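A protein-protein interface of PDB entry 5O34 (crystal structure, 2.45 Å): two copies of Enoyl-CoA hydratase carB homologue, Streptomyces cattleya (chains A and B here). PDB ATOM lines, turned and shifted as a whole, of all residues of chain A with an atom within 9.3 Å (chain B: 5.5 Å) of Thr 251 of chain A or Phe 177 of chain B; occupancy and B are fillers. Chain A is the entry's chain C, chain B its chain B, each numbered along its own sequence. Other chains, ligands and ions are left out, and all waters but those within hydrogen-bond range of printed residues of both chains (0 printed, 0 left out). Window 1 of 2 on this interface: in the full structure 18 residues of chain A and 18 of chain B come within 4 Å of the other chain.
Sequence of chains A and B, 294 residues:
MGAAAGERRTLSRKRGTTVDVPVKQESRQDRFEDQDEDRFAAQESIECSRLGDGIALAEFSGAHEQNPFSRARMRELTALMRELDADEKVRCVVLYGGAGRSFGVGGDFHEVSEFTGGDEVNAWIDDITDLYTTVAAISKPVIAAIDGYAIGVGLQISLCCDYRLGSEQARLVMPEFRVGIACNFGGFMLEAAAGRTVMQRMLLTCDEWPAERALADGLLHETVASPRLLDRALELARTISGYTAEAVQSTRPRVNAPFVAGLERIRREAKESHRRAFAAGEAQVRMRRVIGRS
N of Cys 183 of chain B lies within hydrogen-bond range of OG1 of Thr 251 of chain A, at 3.0 Å. The guanidinium group (NH1) of Arg 254 of chain A lies close to the side-chain amide nitrogen (ND2) of Asn 184 of chain B, at 3.4 Å. The side-chain hydroxyl (OH) of Tyr 243 of chain A lies within hydrogen-bond range of the backbone carbonyl oxygen (O) of Leu 204 of chain B (2.8 Å). SG of Cys 206 of chain B is in hydrogen-bond range of OH of Tyr 243 of chain A, 3.5 Å away.
The backbone carbonyl oxygen (O) of Glu 176 of chain B sits at hydrogen-bond distance from the backbone NH (N) of Ile 181 of chain B, at 2.9 Å. OE1 of Glu 176 of chain B lies within hydrogen-bond range of SG of Cys 183 of chain B. The backbone carbonyl oxygen of Cys 206 of chain B is in hydrogen-bond range of the guanidinium group of Arg 178 of chain B, at 3.0 Å. The side-chain hydroxyl (OG) of Ser 250 of chain A sits at hydrogen-bond distance from the backbone carbonyl oxygen (O) of Glu 246 of chain A (2.9 Å).
Asp 162 of chain A touches Leu 204 of chain B (CB to CD1, 3.8 Å). Phe 177 of chain B touches Ala 247 of chain A. Gly 180 of chain B touches Ala 247 of chain A. Ala 247 of chain A touches Ile 181 of chain B. Ala 182 of chain B touches Ala 247 of chain A. Val 248 of chain A touches Phe 177 of chain B (CG2 to CD1, 3.8 Å). Ser 250 of chain A touches Ala 182 of chain B. ND2 of Asn 184 of chain B touches O of Ser 250 of chain A (3.5 Å). Phe 177 of chain B touches Thr 251 of chain A. Thr 251 of chain A touches Asn 184 of chain B (CA to OD1, 3.5 Å).
Of the printed residues of chain B, Asp 162 of chain A touches Leu 204. Of the printed residues of chain B, Tyr 243 of chain A touches Phe 177, Arg 178, Leu 204 and Cys 206. Thr 251 of chain A touches just these residues of chain B: Phe 177 (3.5 Å), Ala 182 (3.4 Å), Cys 183 (3.0 Å) and Asn 184 (3.5 Å). Of the printed residues of chain A, Phe 177 of chain B touches Tyr 243 (3.7 Å), Ala 247 (3.6 Å), Val 248 (3.8 Å) and Thr 251 (3.5 Å). Printed residues of chain A within 4 Å of Ile 181 of chain B: Ala 247. Ala 182 of chain B touches just these residues of chain A: Ala 247 (3.7 Å), Ser 250 (3.7 Å) and Thr 251 (3.4 Å). Printed residues of chain A within 4 Å of Asn 184 of chain B: Ser 250, Thr 251 and Arg 254. Printed residues of chain A within 4 Å of Leu 204 of chain B: Asp 162 and Tyr 243. The nearest residue of chain A that does not touch Phe 177 of chain B is Thr 244 of chain A (4.4 Å).
Printed residues of chain A that touch a printed residue of chain B: Asp 162, Tyr 243, Thr 244, Ala 247, Val 248, Ser 250, Thr 251 and Arg 254. Of the 14 printed residues of chain B, 9 touch a printed residue of chain A. Printed residues of chain B that touch a printed residue of chain A: Phe 177, Arg 178, Gly 180, Ile 181, Ala 182, Cys 183, Asn 184, Leu 204 and Cys 206. Among the printed residues, 18 pairs touch across the chains.
No position is printed for both chains.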
ATOM      1  N   ALA A 136      27.626  21.172  39.165  1.00  0.00           N
ATOM      2  CA  ALA A 136      26.990  20.465  38.049  1.00  0.00           C
ATOM      3  C   ALA A 136      25.459  20.287  38.176  1.00  0.00           C
ATOM      4  O   ALA A 136      24.782  20.249  37.150  1.00  0.00           O
ATOM      5  CB  ALA A 136      27.663  19.118  37.831  1.00  0.00           C
ATOM      6  N   ALA A 137      24.912  20.212  39.413  1.00  0.00           N
ATOM      7  CA  ALA A 137      23.477  19.971  39.653  1.00  0.00           C
ATOM      8  C   ALA A 137      22.577  21.221  39.726  1.00  0.00           C
ATOM      9  O   ALA A 137      21.370  21.072  39.509  1.00  0.00           O
ATOM     10  CB  ALA A 137      23.272  19.121  40.900  1.00  0.00           C
ATOM     11  N   ILE A 138      23.122  22.431  40.017  1.00  0.00           N
ATOM     12  CA  ILE A 138      22.286  23.649  40.101  1.00  0.00           C
ATOM     13  C   ILE A 138      21.554  23.919  38.767  1.00  0.00           C
ATOM     14  O   ILE A 138      22.017  23.472  37.722  1.00  0.00           O
ATOM     15  CB  ILE A 138      23.022  24.905  40.652  1.00  0.00           C
ATOM     16  CG1 ILE A 138      24.167  25.384  39.730  1.00  0.00           C
ATOM     17  CG2 ILE A 138      23.498  24.670  42.090  1.00  0.00           C
ATOM     18  CD1 ILE A 138      24.487  26.902  39.862  1.00  0.00           C
ATOM     19  N   SER A 139      20.381  24.574  38.818  1.00  0.00           N
ATOM     20  CA  SER A 139      19.572  24.814  37.623  1.00  0.00           C
ATOM     21  C   SER A 139      20.152  25.889  36.692  1.00  0.00           C
ATOM     22  O   SER A 139      19.888  25.856  35.486  1.00  0.00           O
ATOM     23  CB  SER A 139      18.121  25.118  37.995  1.00  0.00           C
ATOM     24  OG  SER A 139      17.967  26.382  38.622  1.00  0.00           O
ATOM     25  N   LYS A 140      20.940  26.828  37.251  1.00  0.00           N
ATOM     26  CA  LYS A 140      21.552  27.948  36.511  1.00  0.00           C
ATOM     27  C   LYS A 140      22.903  27.613  35.881  1.00  0.00           C
ATOM     28  O   LYS A 140      23.696  26.882  36.483  1.00  0.00           O
ATOM     29  CB  LYS A 140      21.722  29.208  37.388  1.00  0.00           C
ATOM     30  CG  LYS A 140      20.791  29.311  38.583  1.00  0.00           C
ATOM     31  CD  LYS A 140      19.844  30.512  38.629  1.00  0.00           C
ATOM     32  CE  LYS A 140      19.076  30.343  39.902  1.00  0.00           C
ATOM     33  NZ  LYS A 140      17.911  31.220  40.042  1.00  0.00           N
ATOM     34  N   PRO A 141      23.218  28.135  34.681  1.00  0.00           N
ATOM     35  CA  PRO A 141      24.521  27.818  34.070  1.00  0.00           C
ATOM     36  C   PRO A 141      25.673  28.574  34.717  1.00  0.00           C
ATOM     37  O   PRO A 141      25.494  29.696  35.207  1.00  0.00           O
ATOM     38  CB  PRO A 141      24.343  28.216  32.601  1.00  0.00           C
ATOM     39  CG  PRO A 141      22.938  28.621  32.459  1.00  0.00           C
ATOM     40  CD  PRO A 141      22.429  29.001  33.800  1.00  0.00           C
ATOM     41  N   ASP A 162      29.495  24.831  32.662  1.00  0.00           N
ATOM     42  CA  ASP A 162      28.888  24.672  31.332  1.00  0.00           C
ATOM     43  C   ASP A 162      29.681  25.311  30.217  1.00  0.00           C
ATOM     44  O   ASP A 162      29.501  24.933  29.061  1.00  0.00           O
ATOM     45  CB  ASP A 162      27.467  25.253  31.318  1.00  0.00           C
ATOM     46  CG  ASP A 162      26.631  24.780  32.474  1.00  0.00           C
ATOM     47  OD1 ASP A 162      25.909  23.775  32.311  1.00  0.00           O
ATOM     48  OD2 ASP A 162      26.750  25.373  33.563  1.00  0.00           O
ATOM     49  N   THR A 239      23.870  37.300  27.622  1.00  0.00           N
ATOM     50  CA  THR A 239      23.170  36.583  26.552  1.00  0.00           C
ATOM     51  C   THR A 239      22.372  35.418  27.159  1.00  0.00           C
ATOM     52  O   THR A 239      21.181  35.283  26.866  1.00  0.00           O
ATOM     53  CB  THR A 239      24.159  36.170  25.441  1.00  0.00           C
ATOM     54  OG1 THR A 239      24.709  37.352  24.856  1.00  0.00           O
ATOM     55  CG2 THR A 239      23.506  35.324  24.334  1.00  0.00           C
ATOM     56  N   ILE A 240      23.018  34.629  28.045  1.00  0.00           N
ATOM     57  CA  ILE A 240      22.401  33.512  28.767  1.00  0.00           C
ATOM     58  C   ILE A 240      21.274  34.018  29.689  1.00  0.00           C
ATOM     59  O   ILE A 240      20.181  33.444  29.686  1.00  0.00           O
ATOM     60  CB  ILE A 240      23.471  32.653  29.502  1.00  0.00           C
ATOM     61  CG1 ILE A 240      24.375  31.907  28.483  1.00  0.00           C
ATOM     62  CG2 ILE A 240      22.826  31.671  30.484  1.00  0.00           C
ATOM     63  CD1 ILE A 240      25.730  31.393  29.038  1.00  0.00           C
ATOM     64  N   SER A 241      21.528  35.126  30.425  1.00  0.00           N
ATOM     65  CA  SER A 241      20.556  35.766  31.322  1.00  0.00           C
ATOM     66  C   SER A 241      19.335  36.278  30.554  1.00  0.00           C
ATOM     67  O   SER A 241      18.243  36.313  31.104  1.00  0.00           O
ATOM     68  CB  SER A 241      21.201  36.920  32.078  1.00  0.00           C
ATOM     69  OG  SER A 241      22.184  36.458  32.991  1.00  0.00           O
ATOM     70  N   GLY A 242      19.539  36.627  29.285  1.00  0.00           N
ATOM     71  CA  GLY A 242      18.498  37.105  28.385  1.00  0.00           C
ATOM     72  C   GLY A 242      17.611  36.023  27.800  1.00  0.00           C
ATOM     73  O   GLY A 242      16.727  36.323  26.995  1.00  0.00           O
ATOM     74  N   TYR A 243      17.853  34.753  28.170  1.00  0.00           N
ATOM     75  CA  TYR A 243      17.044  33.624  27.716  1.00  0.00           C
ATOM     76  C   TYR A 243      15.996  33.358  28.782  1.00  0.00           C
ATOM     77  O   TYR A 243      16.289  33.509  29.978  1.00  0.00           O
ATOM     78  CB  TYR A 243      17.890  32.345  27.555  1.00  0.00           C
ATOM     79  CG  TYR A 243      19.003  32.367  26.527  1.00  0.00           C
ATOM     80  CD1 TYR A 243      18.860  33.064  25.329  1.00  0.00           C
ATOM     81  CD2 TYR A 243      20.147  31.589  26.695  1.00  0.00           C
ATOM     82  CE1 TYR A 243      19.860  33.046  24.358  1.00  0.00           C
ATOM     83  CE2 TYR A 243      21.157  31.567  25.732  1.00  0.00           C
ATOM     84  CZ  TYR A 243      21.008  32.295  24.564  1.00  0.00           C
ATOM     85  OH  TYR A 243      21.987  32.268  23.601  1.00  0.00           O
ATOM     86  N   THR A 244      14.791  32.922  28.352  1.00  0.00           N
ATOM     87  CA  THR A 244      13.664  32.563  29.220  1.00  0.00           C
ATOM     88  C   THR A 244      14.187  31.605  30.277  1.00  0.00           C
ATOM     89  O   THR A 244      14.585  30.483  29.948  1.00  0.00           O
ATOM     90  CB  THR A 244      12.513  31.975  28.380  1.00  0.00           C
ATOM     91  OG1 THR A 244      12.090  32.953  27.425  1.00  0.00           O
ATOM     92  CG2 THR A 244      11.326  31.521  29.230  1.00  0.00           C
ATOM     93  N   ALA A 245      14.286  32.100  31.522  1.00  0.00           N
ATOM     94  CA  ALA A 245      14.796  31.374  32.678  1.00  0.00           C
ATOM     95  C   ALA A 245      14.373  29.903  32.681  1.00  0.00           C
ATOM     96  O   ALA A 245      15.246  29.034  32.713  1.00  0.00           O
ATOM     97  CB  ALA A 245      14.351  32.060  33.959  1.00  0.00           C
ATOM     98  N   GLU A 246      13.040  29.638  32.568  1.00  0.00           N
ATOM     99  CA  GLU A 246      12.402  28.312  32.559  1.00  0.00           C
ATOM    100  C   GLU A 246      13.036  27.351  31.541  1.00  0.00           C
ATOM    101  O   GLU A 246      13.320  26.207  31.888  1.00  0.00           O
ATOM    102  CB  GLU A 246      10.875  28.452  32.332  1.00  0.00           C
ATOM    103  CG  GLU A 246      10.096  27.144  32.183  1.00  0.00           C
ATOM    104  CD  GLU A 246       9.592  26.462  33.447  1.00  0.00           C
ATOM    105  OE1 GLU A 246       8.442  25.969  33.421  1.00  0.00           O
ATOM    106  OE2 GLU A 246      10.345  26.387  34.445  1.00  0.00           O
ATOM    107  N   ALA A 247      13.265  27.823  30.304  1.00  0.00           N
ATOM    108  CA  ALA A 247      13.850  27.043  29.217  1.00  0.00           C
ATOM    109  C   ALA A 247      15.252  26.511  29.560  1.00  0.00           C
ATOM    110  O   ALA A 247      15.507  25.312  29.420  1.00  0.00           O
ATOM    111  CB  ALA A 247      13.902  27.884  27.959  1.00  0.00           C
ATOM    112  N   VAL A 248      16.136  27.406  30.032  1.00  0.00           N
ATOM    113  CA  VAL A 248      17.517  27.114  30.420  1.00  0.00           C
ATOM    114  C   VAL A 248      17.544  26.241  31.687  1.00  0.00           C
ATOM    115  O   VAL A 248      18.180  25.181  31.694  1.00  0.00           O
ATOM    116  CB  VAL A 248      18.313  28.439  30.620  1.00  0.00           C
ATOM    117  CG1 VAL A 248      19.697  28.183  31.190  1.00  0.00           C
ATOM    118  CG2 VAL A 248      18.404  29.232  29.324  1.00  0.00           C
ATOM    119  N   GLN A 249      16.834  26.689  32.743  1.00  0.00           N
ATOM    120  CA  GLN A 249      16.795  26.058  34.067  1.00  0.00           C
ATOM    121  C   GLN A 249      16.065  24.708  34.114  1.00  0.00           C
ATOM    122  O   GLN A 249      16.191  23.998  35.121  1.00  0.00           O
ATOM    123  CB  GLN A 249      16.251  27.028  35.121  1.00  0.00           C
ATOM    124  CG  GLN A 249      17.193  28.213  35.344  1.00  0.00           C
ATOM    125  CD  GLN A 249      16.623  29.312  36.202  1.00  0.00           C
ATOM    126  OE1 GLN A 249      16.672  30.493  35.840  1.00  0.00           O
ATOM    127  NE2 GLN A 249      16.149  28.959  37.395  1.00  0.00           N
ATOM    128  N   SER A 250      15.352  24.327  33.038  1.00  0.00           N
ATOM    129  CA  SER A 250      14.717  23.007  32.963  1.00  0.00           C
ATOM    130  C   SER A 250      15.529  22.057  32.060  1.00  0.00           C
ATOM    131  O   SER A 250      15.250  20.857  32.038  1.00  0.00           O
ATOM    132  CB  SER A 250      13.255  23.103  32.524  1.00  0.00           C
ATOM    133  OG  SER A 250      13.116  23.457  31.158  1.00  0.00           O
ATOM    134  N   THR A 251      16.544  22.592  31.335  1.00  0.00           N
ATOM    135  CA  THR A 251      17.430  21.815  30.463  1.00  0.00           C
ATOM    136  C   THR A 251      18.710  21.400  31.206  1.00  0.00           C
ATOM    137  O   THR A 251      19.065  20.218  31.197  1.00  0.00           O
ATOM    138  CB  THR A 251      17.734  22.577  29.152  1.00  0.00           C
ATOM    139  OG1 THR A 251      16.508  22.962  28.534  1.00  0.00           O
ATOM    140  CG2 THR A 251      18.558  21.751  28.155  1.00  0.00           C
ATOM    141  N   ARG A 252      19.396  22.378  31.840  1.00  0.00           N
ATOM    142  CA  ARG A 252      20.683  22.203  32.518  1.00  0.00           C
ATOM    143  C   ARG A 252      20.736  21.059  33.567  1.00  0.00           C
ATOM    144  O   ARG A 252      21.640  20.236  33.445  1.00  0.00           O
ATOM    145  CB  ARG A 252      21.181  23.523  33.131  1.00  0.00           C
ATOM    146  CG  ARG A 252      22.684  23.580  33.298  1.00  0.00           C
ATOM    147  CD  ARG A 252      23.085  23.775  34.736  1.00  0.00           C
ATOM    148  NE  ARG A 252      24.525  23.995  34.845  1.00  0.00           N
ATOM    149  CZ  ARG A 252      25.258  23.715  35.916  1.00  0.00           C
ATOM    150  NH1 ARG A 252      24.691  23.202  37.001  1.00  0.00           N
ATOM    151  NH2 ARG A 252      26.564  23.938  35.908  1.00  0.00           N
ATOM    152  N   PRO A 253      19.864  20.953  34.598  1.00  0.00           N
ATOM    153  CA  PRO A 253      20.040  19.841  35.556  1.00  0.00           C
ATOM    154  C   PRO A 253      19.794  18.456  34.957  1.00  0.00           C
ATOM    155  O   PRO A 253      20.437  17.481  35.362  1.00  0.00           O
ATOM    156  CB  PRO A 253      19.069  20.182  36.690  1.00  0.00           C
ATOM    157  CG  PRO A 253      18.037  21.041  36.063  1.00  0.00           C
ATOM    158  CD  PRO A 253      18.722  21.815  34.973  1.00  0.00           C
ATOM    159  N   ARG A 254      18.912  18.383  33.954  1.00  0.00           N
ATOM    160  CA  ARG A 254      18.570  17.141  33.267  1.00  0.00           C
ATOM    161  C   ARG A 254      19.668  16.664  32.314  1.00  0.00           C
ATOM    162  O   ARG A 254      19.980  15.469  32.293  1.00  0.00           O
ATOM    163  CB  ARG A 254      17.214  17.270  32.572  1.00  0.00           C
ATOM    164  CG  ARG A 254      16.055  17.001  33.538  1.00  0.00           C
ATOM    165  CD  ARG A 254      14.704  17.359  32.959  1.00  0.00           C
ATOM    166  NE  ARG A 254      14.418  16.613  31.730  1.00  0.00           N
ATOM    167  CZ  ARG A 254      13.399  16.871  30.915  1.00  0.00           C
ATOM    168  NH1 ARG A 254      12.548  17.852  31.193  1.00  0.00           N
ATOM    169  NH2 ARG A 254      13.223  16.148  29.816  1.00  0.00           N
ATOM    170  N   VAL A 255      20.278  17.599  31.566  1.00  0.00           N
ATOM    171  CA  VAL A 255      21.390  17.324  30.652  1.00  0.00           C
ATOM    172  C   VAL A 255      22.661  16.929  31.462  1.00  0.00           C
ATOM    173  O   VAL A 255      23.464  16.120  30.988  1.00  0.00           O
ATOM    174  CB  VAL A 255      21.579  18.502  29.651  1.00  0.00           C
ATOM    175  CG1 VAL A 255      23.021  18.646  29.171  1.00  0.00           C
ATOM    176  CG2 VAL A 255      20.622  18.375  28.470  1.00  0.00           C
ATOM    177  N   ASN A 256      22.777  17.430  32.709  1.00  0.00           N
ATOM    178  CA  ASN A 256      23.890  17.114  33.613  1.00  0.00           C
ATOM    179  C   ASN A 256      23.626  15.962  34.591  1.00  0.00           C
ATOM    180  O   ASN A 256      24.519  15.660  35.386  1.00  0.00           O
ATOM    181  CB  ASN A 256      24.354  18.363  34.385  1.00  0.00           C
ATOM    182  CG  ASN A 256      25.072  19.388  33.535  1.00  0.00           C
ATOM    183  OD1 ASN A 256      25.282  19.220  32.329  1.00  0.00           O
ATOM    184  ND2 ASN A 256      25.450  20.484  34.146  1.00  0.00           N
ATOM    185  N   ALA A 257      22.440  15.310  34.534  1.00  0.00           N
ATOM    186  CA  ALA A 257      22.125  14.171  35.419  1.00  0.00           C
ATOM    187  C   ALA A 257      23.117  12.986  35.245  1.00  0.00           C
ATOM    188  O   ALA A 257      23.718  12.600  36.251  1.00  0.00           O
ATOM    189  CB  ALA A 257      20.678  13.717  35.245  1.00  0.00           C
ATOM    190  N   PRO A 258      23.387  12.456  34.015  1.00  0.00           N
ATOM    191  CA  PRO A 258      24.401  11.376  33.878  1.00  0.00           C
ATOM    192  C   PRO A 258      25.785  11.706  34.462  1.00  0.00           C
ATOM    193  O   PRO A 258      26.417  10.840  35.075  1.00  0.00           O
ATOM    194  CB  PRO A 258      24.487  11.164  32.363  1.00  0.00           C
ATOM    195  CG  PRO A 258      23.170  11.622  31.843  1.00  0.00           C
ATOM    196  CD  PRO A 258      22.788  12.784  32.700  1.00  0.00           C
ATOM    197  N   MET B 174      20.961  25.236  16.804  1.00  0.00           N
ATOM    198  CA  MET B 174      20.138  24.682  17.885  1.00  0.00           C
ATOM    199  C   MET B 174      19.792  25.899  18.754  1.00  0.00           C
ATOM    200  O   MET B 174      20.417  26.123  19.801  1.00  0.00           O
ATOM    201  CB  MET B 174      20.884  23.582  18.667  1.00  0.00           C
ATOM    202  CG  MET B 174      19.951  22.614  19.397  1.00  0.00           C
ATOM    203  SD  MET B 174      18.926  21.562  18.318  1.00  0.00           S
ATOM    204  CE  MET B 174      20.008  20.150  18.128  1.00  0.00           C
ATOM    205  N   PRO B 175      18.858  26.764  18.268  1.00  0.00           N
ATOM    206  CA  PRO B 175      18.592  28.032  18.962  1.00  0.00           C
ATOM    207  C   PRO B 175      17.411  28.031  19.929  1.00  0.00           C
ATOM    208  O   PRO B 175      16.900  29.107  20.255  1.00  0.00           O
ATOM    209  CB  PRO B 175      18.366  28.997  17.797  1.00  0.00           C
ATOM    210  CG  PRO B 175      17.764  28.133  16.703  1.00  0.00           C
ATOM    211  CD  PRO B 175      18.053  26.678  17.030  1.00  0.00           C
ATOM    212  N   GLU B 176      17.003  26.831  20.411  1.00  0.00           N
ATOM    213  CA  GLU B 176      15.894  26.601  21.350  1.00  0.00           C
ATOM    214  C   GLU B 176      15.807  27.599  22.512  1.00  0.00           C
ATOM    215  O   GLU B 176      14.700  28.028  22.845  1.00  0.00           O
ATOM    216  CB  GLU B 176      15.943  25.167  21.890  1.00  0.00           C
ATOM    217  CG  GLU B 176      15.256  24.137  21.012  1.00  0.00           C
ATOM    218  CD  GLU B 176      15.962  23.700  19.742  1.00  0.00           C
ATOM    219  OE1 GLU B 176      17.115  24.123  19.502  1.00  0.00           O
ATOM    220  OE2 GLU B 176      15.343  22.930  18.975  1.00  0.00           O
ATOM    221  N   PHE B 177      16.961  27.964  23.123  1.00  0.00           N
ATOM    222  CA  PHE B 177      17.041  28.916  24.240  1.00  0.00           C
ATOM    223  C   PHE B 177      16.658  30.346  23.817  1.00  0.00           C
ATOM    224  O   PHE B 177      15.868  30.984  24.511  1.00  0.00           O
ATOM    225  CB  PHE B 177      18.429  28.884  24.918  1.00  0.00           C
ATOM    226  CG  PHE B 177      18.754  27.691  25.802  1.00  0.00           C
ATOM    227  CD1 PHE B 177      20.022  27.541  26.358  1.00  0.00           C
ATOM    228  CD2 PHE B 177      17.792  26.723  26.084  1.00  0.00           C
ATOM    229  CE1 PHE B 177      20.318  26.455  27.189  1.00  0.00           C
ATOM    230  CE2 PHE B 177      18.098  25.625  26.899  1.00  0.00           C
ATOM    231  CZ  PHE B 177      19.356  25.502  27.451  1.00  0.00           C
ATOM    232  N   ARG B 178      17.192  30.835  22.667  1.00  0.00           N
ATOM    233  CA  ARG B 178      16.871  32.161  22.110  1.00  0.00           C
ATOM    234  C   ARG B 178      15.373  32.241  21.725  1.00  0.00           C
ATOM    235  O   ARG B 178      14.748  33.288  21.887  1.00  0.00           O
ATOM    236  CB  ARG B 178      17.799  32.510  20.929  1.00  0.00           C
ATOM    237  CG  ARG B 178      17.343  33.716  20.101  1.00  0.00           C
ATOM    238  CD  ARG B 178      18.450  34.459  19.366  1.00  0.00           C
ATOM    239  NE  ARG B 178      19.357  33.594  18.604  1.00  0.00           N
ATOM    240  CZ  ARG B 178      19.047  32.951  17.478  1.00  0.00           C
ATOM    241  NH1 ARG B 178      17.813  33.018  16.984  1.00  0.00           N
ATOM    242  NH2 ARG B 178      19.955  32.213  16.855  1.00  0.00           N
ATOM    243  N   VAL B 179      14.804  31.109  21.285  1.00  0.00           N
ATOM    244  CA  VAL B 179      13.397  30.935  20.924  1.00  0.00           C
ATOM    245  C   VAL B 179      12.507  30.858  22.204  1.00  0.00           C
ATOM    246  O   VAL B 179      11.316  31.162  22.139  1.00  0.00           O
ATOM    247  CB  VAL B 179      13.258  29.731  19.941  1.00  0.00           C
ATOM    248  CG1 VAL B 179      11.882  29.068  19.985  1.00  0.00           C
ATOM    249  CG2 VAL B 179      13.607  30.159  18.519  1.00  0.00           C
ATOM    250  N   GLY B 180      13.114  30.504  23.340  1.00  0.00           N
ATOM    251  CA  GLY B 180      12.459  30.453  24.646  1.00  0.00           C
ATOM    252  C   GLY B 180      11.950  29.111  25.141  1.00  0.00           C
ATOM    253  O   GLY B 180      11.191  29.068  26.118  1.00  0.00           O
ATOM    254  N   ILE B 181      12.371  28.003  24.497  1.00  0.00           N
ATOM    255  CA  ILE B 181      11.947  26.635  24.852  1.00  0.00           C
ATOM    256  C   ILE B 181      13.119  25.739  25.303  1.00  0.00           C
ATOM    257  O   ILE B 181      14.271  25.992  24.939  1.00  0.00           O
ATOM    258  CB  ILE B 181      11.117  25.976  23.707  1.00  0.00           C
ATOM    259  CG1 ILE B 181      11.950  25.814  22.408  1.00  0.00           C
ATOM    260  CG2 ILE B 181       9.812  26.759  23.452  1.00  0.00           C
ATOM    261  CD1 ILE B 181      11.386  24.846  21.383  1.00  0.00           C
ATOM    262  N   ALA B 182      12.811  24.686  26.085  1.00  0.00           N
ATOM    263  CA  ALA B 182      13.792  23.723  26.587  1.00  0.00           C
ATOM    264  C   ALA B 182      14.477  22.960  25.432  1.00  0.00           C
ATOM    265  O   ALA B 182      13.960  22.939  24.307  1.00  0.00           O
ATOM    266  CB  ALA B 182      13.131  22.756  27.562  1.00  0.00           C
ATOM    267  N   CYS B 183      15.650  22.375  25.697  1.00  0.00           N
ATOM    268  CA  CYS B 183      16.404  21.669  24.668  1.00  0.00           C
ATOM    269  C   CYS B 183      16.955  20.355  25.214  1.00  0.00           C
ATOM    270  O   CYS B 183      18.157  20.086  25.152  1.00  0.00           O
ATOM    271  CB  CYS B 183      17.504  22.565  24.101  1.00  0.00           C
ATOM    272  SG  CYS B 183      18.019  22.120  22.423  1.00  0.00           S
ATOM    273  N   ASN B 184      16.055  19.534  25.763  1.00  0.00           N
ATOM    274  CA  ASN B 184      16.410  18.257  26.356  1.00  0.00           C
ATOM    275  C   ASN B 184      16.735  17.205  25.307  1.00  0.00           C
ATOM    276  O   ASN B 184      17.719  16.491  25.477  1.00  0.00           O
ATOM    277  CB  ASN B 184      15.362  17.812  27.361  1.00  0.00           C
ATOM    278  CG  ASN B 184      15.472  18.632  28.632  1.00  0.00           C
ATOM    279  OD1 ASN B 184      16.498  18.610  29.333  1.00  0.00           O
ATOM    280  ND2 ASN B 184      14.463  19.444  28.907  1.00  0.00           N
ATOM    281  N   LEU B 203      24.091  25.236  22.355  1.00  0.00           N
ATOM    282  CA  LEU B 203      22.938  25.612  23.174  1.00  0.00           C
ATOM    283  C   LEU B 203      23.048  27.006  23.780  1.00  0.00           C
ATOM    284  O   LEU B 203      22.110  27.792  23.659  1.00  0.00           O
ATOM    285  CB  LEU B 203      22.695  24.600  24.315  1.00  0.00           C
ATOM    286  CG  LEU B 203      22.223  23.169  23.996  1.00  0.00           C
ATOM    287  CD1 LEU B 203      21.295  22.659  25.084  1.00  0.00           C
ATOM    288  CD2 LEU B 203      21.578  23.055  22.638  1.00  0.00           C
ATOM    289  N   LEU B 204      24.178  27.303  24.445  1.00  0.00           N
ATOM    290  CA  LEU B 204      24.383  28.566  25.146  1.00  0.00           C
ATOM    291  C   LEU B 204      24.630  29.768  24.248  1.00  0.00           C
ATOM    292  O   LEU B 204      24.203  30.859  24.612  1.00  0.00           O
ATOM    293  CB  LEU B 204      25.488  28.432  26.199  1.00  0.00           C
ATOM    294  CG  LEU B 204      25.223  27.347  27.249  1.00  0.00           C
ATOM    295  CD1 LEU B 204      26.402  27.169  28.158  1.00  0.00           C
ATOM    296  CD2 LEU B 204      23.962  27.645  28.065  1.00  0.00           C
ATOM    297  N   CYS B 206      23.728  29.885  20.799  1.00  0.00           N
ATOM    298  CA  CYS B 206      22.681  29.869  19.764  1.00  0.00           C
ATOM    299  C   CYS B 206      23.206  30.307  18.390  1.00  0.00           C
ATOM    300  O   CYS B 206      22.417  30.600  17.490  1.00  0.00           O
ATOM    301  CB  CYS B 206      21.443  30.656  20.188  1.00  0.00           C
ATOM    302  SG  CYS B 206      20.538  29.890  21.555  1.00  0.00           S
